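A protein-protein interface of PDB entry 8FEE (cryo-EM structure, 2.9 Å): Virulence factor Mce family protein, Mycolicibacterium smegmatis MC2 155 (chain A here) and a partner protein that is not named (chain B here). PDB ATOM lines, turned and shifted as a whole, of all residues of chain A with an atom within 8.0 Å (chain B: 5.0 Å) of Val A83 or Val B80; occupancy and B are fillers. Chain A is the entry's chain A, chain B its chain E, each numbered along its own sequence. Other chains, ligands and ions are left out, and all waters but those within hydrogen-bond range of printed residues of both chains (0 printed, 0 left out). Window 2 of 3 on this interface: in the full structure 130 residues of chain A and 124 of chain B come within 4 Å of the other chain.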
ATOM      1  N   LEU A  54       6.436   3.840  -3.776  1.00  0.00           N
ATOM      2  CA  LEU A  54       6.862   3.534  -5.132  1.00  0.00           C
ATOM      3  C   LEU A  54       6.619   2.060  -5.420  1.00  0.00           C
ATOM      4  O   LEU A  54       6.855   1.204  -4.562  1.00  0.00           O
ATOM      5  CB  LEU A  54       8.338   3.880  -5.338  1.00  0.00           C
ATOM      6  CG  LEU A  54       8.669   5.372  -5.387  1.00  0.00           C
ATOM      7  CD1 LEU A  54      10.146   5.603  -5.129  1.00  0.00           C
ATOM      8  CD2 LEU A  54       8.265   5.961  -6.726  1.00  0.00           C
ATOM      9  N   GLY A  56       6.315  -1.002  -8.954  1.00  0.00           N
ATOM     10  CA  GLY A  56       6.498  -1.264 -10.371  1.00  0.00           C
ATOM     11  C   GLY A  56       5.260  -0.930 -11.180  1.00  0.00           C
ATOM     12  O   GLY A  56       5.352  -0.327 -12.252  1.00  0.00           O
ATOM     13  N   ALA A  58       0.877   0.265 -10.542  1.00  0.00           N
ATOM     14  CA  ALA A  58      -0.107   0.707  -9.559  1.00  0.00           C
ATOM     15  C   ALA A  58      -1.111  -0.392  -9.239  1.00  0.00           C
ATOM     16  O   ALA A  58      -1.512  -0.556  -8.082  1.00  0.00           O
ATOM     17  CB  ALA A  58      -0.828   1.956 -10.060  1.00  0.00           C
ATOM     18  N   ILE A  81      -2.104   9.071  -7.768  1.00  0.00           N
ATOM     19  CA  ILE A  81      -1.183   8.154  -8.430  1.00  0.00           C
ATOM     20  C   ILE A  81      -0.586   8.853  -9.644  1.00  0.00           C
ATOM     21  O   ILE A  81      -1.302   9.513 -10.405  1.00  0.00           O
ATOM     22  CB  ILE A  81      -1.867   6.839  -8.858  1.00  0.00           C
ATOM     23  CG1 ILE A  81      -2.766   6.297  -7.749  1.00  0.00           C
ATOM     24  CG2 ILE A  81      -0.828   5.799  -9.233  1.00  0.00           C
ATOM     25  CD1 ILE A  81      -3.438   5.001  -8.107  1.00  0.00           C
ATOM     26  N   ASP A  82       0.725   8.707  -9.825  1.00  0.00           N
ATOM     27  CA  ASP A  82       1.443   9.362 -10.910  1.00  0.00           C
ATOM     28  C   ASP A  82       2.457   8.384 -11.487  1.00  0.00           C
ATOM     29  O   ASP A  82       2.761   7.348 -10.892  1.00  0.00           O
ATOM     30  CB  ASP A  82       2.129  10.647 -10.426  1.00  0.00           C
ATOM     31  CG  ASP A  82       2.459  11.601 -11.560  1.00  0.00           C
ATOM     32  OD1 ASP A  82       2.609  11.141 -12.712  1.00  0.00           O
ATOM     33  OD2 ASP A  82       2.569  12.818 -11.298  1.00  0.00           O
ATOM     34  N   VAL A  83       2.983   8.718 -12.663  1.00  0.00           N
ATOM     35  CA  VAL A  83       3.986   7.905 -13.345  1.00  0.00           C
ATOM     36  C   VAL A  83       5.312   8.653 -13.307  1.00  0.00           C
ATOM     37  O   VAL A  83       5.408   9.787 -13.793  1.00  0.00           O
ATOM     38  CB  VAL A  83       3.574   7.588 -14.791  1.00  0.00           C
ATOM     39  CG1 VAL A  83       4.754   7.032 -15.569  1.00  0.00           C
ATOM     40  CG2 VAL A  83       2.425   6.604 -14.805  1.00  0.00           C
ATOM     41  N   VAL A  84       6.334   8.019 -12.736  1.00  0.00           N
ATOM     42  CA  VAL A  84       7.644   8.630 -12.539  1.00  0.00           C
ATOM     43  C   VAL A  84       8.666   7.858 -13.358  1.00  0.00           C
ATOM     44  O   VAL A  84       8.715   6.623 -13.295  1.00  0.00           O
ATOM     45  CB  VAL A  84       8.043   8.654 -11.054  1.00  0.00           C
ATOM     46  CG1 VAL A  84       9.314   9.462 -10.862  1.00  0.00           C
ATOM     47  CG2 VAL A  84       6.923   9.238 -10.233  1.00  0.00           C
ATOM     48  N   GLU A  85       9.474   8.582 -14.129  1.00  0.00           N
ATOM     49  CA  GLU A  85      10.490   7.971 -14.984  1.00  0.00           C
ATOM     50  C   GLU A  85      11.740   7.748 -14.142  1.00  0.00           C
ATOM     51  O   GLU A  85      12.631   8.597 -14.075  1.00  0.00           O
ATOM     52  CB  GLU A  85      10.774   8.853 -16.194  1.00  0.00           C
ATOM     53  CG  GLU A  85      11.665   8.214 -17.246  1.00  0.00           C
ATOM     54  CD  GLU A  85      10.901   7.287 -18.173  1.00  0.00           C
ATOM     55  OE1 GLU A  85       9.657   7.242 -18.083  1.00  0.00           O
ATOM     56  OE2 GLU A  85      11.547   6.607 -18.997  1.00  0.00           O
ATOM     57  N   VAL A  86      11.809   6.592 -13.489  1.00  0.00           N
ATOM     58  CA  VAL A  86      12.948   6.223 -12.658  1.00  0.00           C
ATOM     59  C   VAL A  86      13.867   5.346 -13.497  1.00  0.00           C
ATOM     60  O   VAL A  86      13.433   4.315 -14.025  1.00  0.00           O
ATOM     61  CB  VAL A  86      12.501   5.496 -11.380  1.00  0.00           C
ATOM     62  CG1 VAL A  86      13.694   5.216 -10.484  1.00  0.00           C
ATOM     63  CG2 VAL A  86      11.456   6.316 -10.643  1.00  0.00           C
ATOM     64  N   ASN A  89      12.612   4.233 -16.811  1.00  0.00           N
ATOM     65  CA  ASN A  89      11.611   3.194 -16.689  1.00  0.00           C
ATOM     66  C   ASN A  89      10.423   3.774 -15.934  1.00  0.00           C
ATOM     67  O   ASN A  89      10.619   4.346 -14.851  1.00  0.00           O
ATOM     68  CB  ASN A  89      12.151   1.966 -15.955  1.00  0.00           C
ATOM     69  CG  ASN A  89      11.254   0.756 -16.106  1.00  0.00           C
ATOM     70  OD1 ASN A  89      10.704   0.508 -17.178  1.00  0.00           O
ATOM     71  ND2 ASN A  89      11.101  -0.004 -15.030  1.00  0.00           N
ATOM     72  N   PRO A  90       9.210   3.681 -16.472  1.00  0.00           N
ATOM     73  CA  PRO A  90       8.051   4.207 -15.743  1.00  0.00           C
ATOM     74  C   PRO A  90       7.727   3.347 -14.533  1.00  0.00           C
ATOM     75  O   PRO A  90       7.730   2.116 -14.602  1.00  0.00           O
ATOM     76  CB  PRO A  90       6.926   4.158 -16.784  1.00  0.00           C
ATOM     77  CG  PRO A  90       7.351   3.091 -17.736  1.00  0.00           C
ATOM     78  CD  PRO A  90       8.845   3.187 -17.809  1.00  0.00           C
ATOM     79  N   GLU A  91       7.454   4.011 -13.412  1.00  0.00           N
ATOM     80  CA  GLU A  91       7.015   3.344 -12.196  1.00  0.00           C
ATOM     81  C   GLU A  91       5.869   4.136 -11.589  1.00  0.00           C
ATOM     82  O   GLU A  91       5.715   5.333 -11.843  1.00  0.00           O
ATOM     83  CB  GLU A  91       8.157   3.193 -11.180  1.00  0.00           C
ATOM     84  CG  GLU A  91       9.345   2.398 -11.690  1.00  0.00           C
ATOM     85  CD  GLU A  91      10.195   1.839 -10.571  1.00  0.00           C
ATOM     86  OE1 GLU A  91       9.917   2.159  -9.396  1.00  0.00           O
ATOM     87  OE2 GLU A  91      11.139   1.076 -10.863  1.00  0.00           O
ATOM     88  N   ALA A  92       5.053   3.458 -10.787  1.00  0.00           N
ATOM     89  CA  ALA A  92       3.894   4.094 -10.183  1.00  0.00           C
ATOM     90  C   ALA A  92       4.273   4.690  -8.835  1.00  0.00           C
ATOM     91  O   ALA A  92       4.897   4.021  -8.003  1.00  0.00           O
ATOM     92  CB  ALA A  92       2.752   3.092 -10.017  1.00  0.00           C
ATOM     93  N   ARG A  93       3.902   5.950  -8.624  1.00  0.00           N
ATOM     94  CA  ARG A  93       4.112   6.642  -7.361  1.00  0.00           C
ATOM     95  C   ARG A  93       2.758   6.994  -6.773  1.00  0.00           C
ATOM     96  O   ARG A  93       1.947   7.654  -7.429  1.00  0.00           O
ATOM     97  CB  ARG A  93       4.946   7.910  -7.554  1.00  0.00           C
ATOM     98  CG  ARG A  93       5.033   8.778  -6.313  1.00  0.00           C
ATOM     99  CD  ARG A  93       6.132   9.819  -6.430  1.00  0.00           C
ATOM    100  NE  ARG A  93       5.883  10.762  -7.511  1.00  0.00           N
ATOM    101  CZ  ARG A  93       5.195  11.888  -7.378  1.00  0.00           C
ATOM    102  NH1 ARG A  93       4.644  12.230  -6.225  1.00  0.00           N
ATOM    103  NH2 ARG A  93       5.049  12.688  -8.431  1.00  0.00           N
ATOM    104  N   LEU A  94       2.516   6.565  -5.542  1.00  0.00           N
ATOM    105  CA  LEU A  94       1.242   6.777  -4.877  1.00  0.00           C
ATOM    106  C   LEU A  94       1.446   7.733  -3.713  1.00  0.00           C
ATOM    107  O   LEU A  94       2.377   7.559  -2.919  1.00  0.00           O
ATOM    108  CB  LEU A  94       0.648   5.458  -4.370  1.00  0.00           C
ATOM    109  CG  LEU A  94       0.132   4.369  -5.321  1.00  0.00           C
ATOM    110  CD1 LEU A  94       1.236   3.696  -6.125  1.00  0.00           C
ATOM    111  CD2 LEU A  94      -0.652   3.332  -4.535  1.00  0.00           C
ATOM    112  N   PRO B  48      -7.067  13.219 -18.099  1.00  0.00           N
ATOM    113  CA  PRO B  48      -5.785  13.125 -18.805  1.00  0.00           C
ATOM    114  C   PRO B  48      -5.970  12.987 -20.309  1.00  0.00           C
ATOM    115  O   PRO B  48      -6.949  12.413 -20.789  1.00  0.00           O
ATOM    116  CB  PRO B  48      -5.147  11.869 -18.207  1.00  0.00           C
ATOM    117  CG  PRO B  48      -5.727  11.783 -16.843  1.00  0.00           C
ATOM    118  CD  PRO B  48      -7.136  12.291 -16.958  1.00  0.00           C
ATOM    119  N   GLY B  49      -5.007  13.527 -21.052  1.00  0.00           N
ATOM    120  CA  GLY B  49      -5.041  13.512 -22.496  1.00  0.00           C
ATOM    121  C   GLY B  49      -5.763  14.680 -23.128  1.00  0.00           C
ATOM    122  O   GLY B  49      -5.714  14.827 -24.355  1.00  0.00           O
ATOM    123  N   VAL B  73      -6.579   4.895 -21.022  1.00  0.00           N
ATOM    124  CA  VAL B  73      -5.290   4.413 -21.493  1.00  0.00           C
ATOM    125  C   VAL B  73      -4.345   4.403 -20.303  1.00  0.00           C
ATOM    126  O   VAL B  73      -4.091   5.447 -19.692  1.00  0.00           O
ATOM    127  CB  VAL B  73      -4.744   5.287 -22.631  1.00  0.00           C
ATOM    128  CG1 VAL B  73      -3.285   4.973 -22.880  1.00  0.00           C
ATOM    129  CG2 VAL B  73      -5.561   5.070 -23.886  1.00  0.00           C
ATOM    130  N   ARG B  74      -3.826   3.229 -19.968  1.00  0.00           N
ATOM    131  CA  ARG B  74      -3.050   3.027 -18.755  1.00  0.00           C
ATOM    132  C   ARG B  74      -1.613   2.669 -19.103  1.00  0.00           C
ATOM    133  O   ARG B  74      -1.368   1.736 -19.875  1.00  0.00           O
ATOM    134  CB  ARG B  74      -3.676   1.932 -17.892  1.00  0.00           C
ATOM    135  CG  ARG B  74      -5.079   2.254 -17.420  1.00  0.00           C
ATOM    136  CD  ARG B  74      -5.593   1.183 -16.488  1.00  0.00           C
ATOM    137  NE  ARG B  74      -6.937   1.471 -16.004  1.00  0.00           N
ATOM    138  CZ  ARG B  74      -7.212   1.951 -14.799  1.00  0.00           C
ATOM    139  NH1 ARG B  74      -6.255   2.226 -13.930  1.00  0.00           N
ATOM    140  NH2 ARG B  74      -8.480   2.162 -14.460  1.00  0.00           N
ATOM    141  N   VAL B  75      -0.671   3.414 -18.534  1.00  0.00           N
ATOM    142  CA  VAL B  75       0.742   3.056 -18.547  1.00  0.00           C
ATOM    143  C   VAL B  75       1.118   2.665 -17.127  1.00  0.00           C
ATOM    144  O   VAL B  75       0.951   3.461 -16.195  1.00  0.00           O
ATOM    145  CB  VAL B  75       1.622   4.207 -19.057  1.00  0.00           C
ATOM    146  CG1 VAL B  75       3.086   3.825 -18.965  1.00  0.00           C
ATOM    147  CG2 VAL B  75       1.252   4.559 -20.485  1.00  0.00           C
ATOM    148  N   VAL B  78      -1.672   2.974 -14.547  1.00  0.00           N
ATOM    149  CA  VAL B  78      -1.987   4.314 -14.065  1.00  0.00           C
ATOM    150  C   VAL B  78      -2.781   5.032 -15.147  1.00  0.00           C
ATOM    151  O   VAL B  78      -2.356   5.079 -16.305  1.00  0.00           O
ATOM    152  CB  VAL B  78      -0.717   5.105 -13.702  1.00  0.00           C
ATOM    153  CG1 VAL B  78      -1.076   6.507 -13.249  1.00  0.00           C
ATOM    154  CG2 VAL B  78       0.072   4.383 -12.630  1.00  0.00           C
ATOM    155  N   PHE B  79      -3.929   5.586 -14.766  1.00  0.00           N
ATOM    156  CA  PHE B  79      -4.836   6.256 -15.695  1.00  0.00           C
ATOM    157  C   PHE B  79      -4.160   7.520 -16.212  1.00  0.00           C
ATOM    158  O   PHE B  79      -4.108   8.541 -15.522  1.00  0.00           O
ATOM    159  CB  PHE B  79      -6.149   6.555 -14.979  1.00  0.00           C
ATOM    160  CG  PHE B  79      -7.067   7.500 -15.709  1.00  0.00           C
ATOM    161  CD1 PHE B  79      -7.261   7.406 -17.076  1.00  0.00           C
ATOM    162  CD2 PHE B  79      -7.762   8.469 -15.008  1.00  0.00           C
ATOM    163  CE1 PHE B  79      -8.116   8.273 -17.727  1.00  0.00           C
ATOM    164  CE2 PHE B  79      -8.617   9.335 -15.655  1.00  0.00           C
ATOM    165  CZ  PHE B  79      -8.794   9.235 -17.016  1.00  0.00           C
ATOM    166  N   VAL B  80      -3.635   7.456 -17.437  1.00  0.00           N
ATOM    167  CA  VAL B  80      -2.792   8.519 -17.977  1.00  0.00           C
ATOM    168  C   VAL B  80      -3.225   8.922 -19.381  1.00  0.00           C
ATOM    169  O   VAL B  80      -2.461   9.563 -20.109  1.00  0.00           O
ATOM    170  CB  VAL B  80      -1.310   8.103 -17.991  1.00  0.00           C
ATOM    171  CG1 VAL B  80      -0.777   7.934 -16.582  1.00  0.00           C
ATOM    172  CG2 VAL B  80      -1.127   6.828 -18.790  1.00  0.00           C
ATOM    173  N   GLY B  81      -4.438   8.558 -19.780  1.00  0.00           N
ATOM    174  CA  GLY B  81      -4.844   8.888 -21.133  1.00  0.00           C
ATOM    175  C   GLY B  81      -6.288   8.525 -21.392  1.00  0.00           C
ATOM    176  O   GLY B  81      -6.981   7.973 -20.535  1.00  0.00           O
ATOM    177  N   ARG B  82      -6.726   8.833 -22.610  1.00  0.00           N
ATOM    178  CA  ARG B  82      -8.097   8.587 -23.029  1.00  0.00           C
ATOM    179  C   ARG B  82      -8.108   8.251 -24.513  1.00  0.00           C
ATOM    180  O   ARG B  82      -7.338   8.825 -25.287  1.00  0.00           O
ATOM    181  CB  ARG B  82      -8.979   9.810 -22.747  1.00  0.00           C
ATOM    182  CG  ARG B  82     -10.453   9.612 -23.028  1.00  0.00           C
ATOM    183  CD  ARG B  82     -11.108  10.933 -23.383  1.00  0.00           C
ATOM    184  NE  ARG B  82     -10.347  11.647 -24.401  1.00  0.00           N
ATOM    185  CZ  ARG B  82     -10.732  12.785 -24.963  1.00  0.00           C
ATOM    186  NH1 ARG B  82     -11.875  13.363 -24.639  1.00  0.00           N
ATOM    187  NH2 ARG B  82      -9.949  13.353 -25.875  1.00  0.00           N
ATOM    188  N   ASP B  98      -5.225   9.712 -26.849  1.00  0.00           N
ATOM    189  CA  ASP B  98      -4.609  10.933 -26.343  1.00  0.00           C
ATOM    190  C   ASP B  98      -3.958  10.625 -25.002  1.00  0.00           C
ATOM    191  O   ASP B  98      -4.631  10.151 -24.080  1.00  0.00           O
ATOM    192  CB  ASP B  98      -5.644  12.047 -26.197  1.00  0.00           C
ATOM    193  CG  ASP B  98      -6.251  12.454 -27.522  1.00  0.00           C
ATOM    194  OD1 ASP B  98      -5.794  11.945 -28.565  1.00  0.00           O
ATOM    195  OD2 ASP B  98      -7.185  13.283 -27.523  1.00  0.00           O
ATOM    196  N   VAL B  99      -2.656  10.891 -24.893  1.00  0.00           N
ATOM    197  CA  VAL B  99      -1.934  10.654 -23.648  1.00  0.00           C
ATOM    198  C   VAL B  99      -1.343  11.971 -23.164  1.00  0.00           C
ATOM    199  O   VAL B  99      -0.934  12.821 -23.961  1.00  0.00           O
ATOM    200  CB  VAL B  99      -0.833   9.581 -23.846  1.00  0.00           C
ATOM    201  CG1 VAL B  99       0.017   9.394 -22.598  1.00  0.00           C
ATOM    202  CG2 VAL B  99      -1.448   8.260 -24.241  1.00  0.00           C
ATOM    203  N   GLU B 100      -1.293  12.128 -21.840  1.00  0.00           N
ATOM    204  CA  GLU B 100      -0.853  13.372 -21.233  1.00  0.00           C
ATOM    205  C   GLU B 100       0.635  13.603 -21.496  1.00  0.00           C
ATOM    206  O   GLU B 100       1.393  12.649 -21.694  1.00  0.00           O
ATOM    207  CB  GLU B 100      -1.123  13.344 -19.731  1.00  0.00           C
ATOM    208  CG  GLU B 100      -0.466  12.186 -19.005  1.00  0.00           C
ATOM    209  CD  GLU B 100      -0.869  12.113 -17.550  1.00  0.00           C
ATOM    210  OE1 GLU B 100      -1.826  12.815 -17.163  1.00  0.00           O
ATOM    211  OE2 GLU B 100      -0.229  11.356 -16.790  1.00  0.00           O
ATOM    212  N   ILE B 103       5.192  11.673 -20.649  1.00  0.00           N
ATOM    213  CA  ILE B 103       5.332  10.223 -20.648  1.00  0.00           C
ATOM    214  C   ILE B 103       6.130   9.818 -21.877  1.00  0.00           C
ATOM    215  O   ILE B 103       5.779  10.194 -23.002  1.00  0.00           O
ATOM    216  CB  ILE B 103       3.965   9.517 -20.626  1.00  0.00           C
ATOM    217  CG1 ILE B 103       3.199   9.898 -19.361  1.00  0.00           C
ATOM    218  CG2 ILE B 103       4.144   8.010 -20.710  1.00  0.00           C
ATOM    219  CD1 ILE B 103       1.982   9.056 -19.113  1.00  0.00           C
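Among the printed residues, pairs that only touch across the chains: Ala A58 with Val B78, Val A83 with Val B78, Val A83 with Val B75, Ile A81 with Val B78, Val A83 with Val B80 and Ala A92 with Val B78.
N of Val B80 lies within hydrogen-bond range of O of Val B73, 3.1 Å away. The backbone NH (N) of Glu B100 is in hydrogen-bond range of the backbone carbonyl oxygen (O) of Val B80 (3.3 Å).
Of the printed residues of chain B, Val A83 touches Val B75, Val B78 and Val B80. Val B80 touches one residue of chain A. Of the printed residues of chain A, Val B75 touches Val A83. Printed residues of chain B within 4 Å of Ile A81: Val B78. Printed residues of chain B within 4 Å of Ala A92: Val B78 (3.96 Å). Printed residues of chain B within 4 Å of Ala A58: Val B78 (3.6 Å). Leu A54 touches none of the printed residues of chain B. The nearest residue of chain A that does not touch Val B80 is Asp A82 (6.1 Å). The nearest printed residue of chain B that does not touch Ile A81 is Phe B79 (5.9 Å).
Of the 15 printed residues of chain A, 4 touch a printed residue of chain B. Printed residues of chain A that touch a printed residue of chain B: Ala A58, Ile A81, Val A83 and Ala A92. Hydrophobic or aromatic side chains of chain A that line the printed part of chain B: Ala A58, Ile A81, Val A83 and Ala A92. Among the printed residues, no Asp or Glu carboxylate lies within 4 Å of a Lys or Arg side-chain nitrogen of the other chain.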
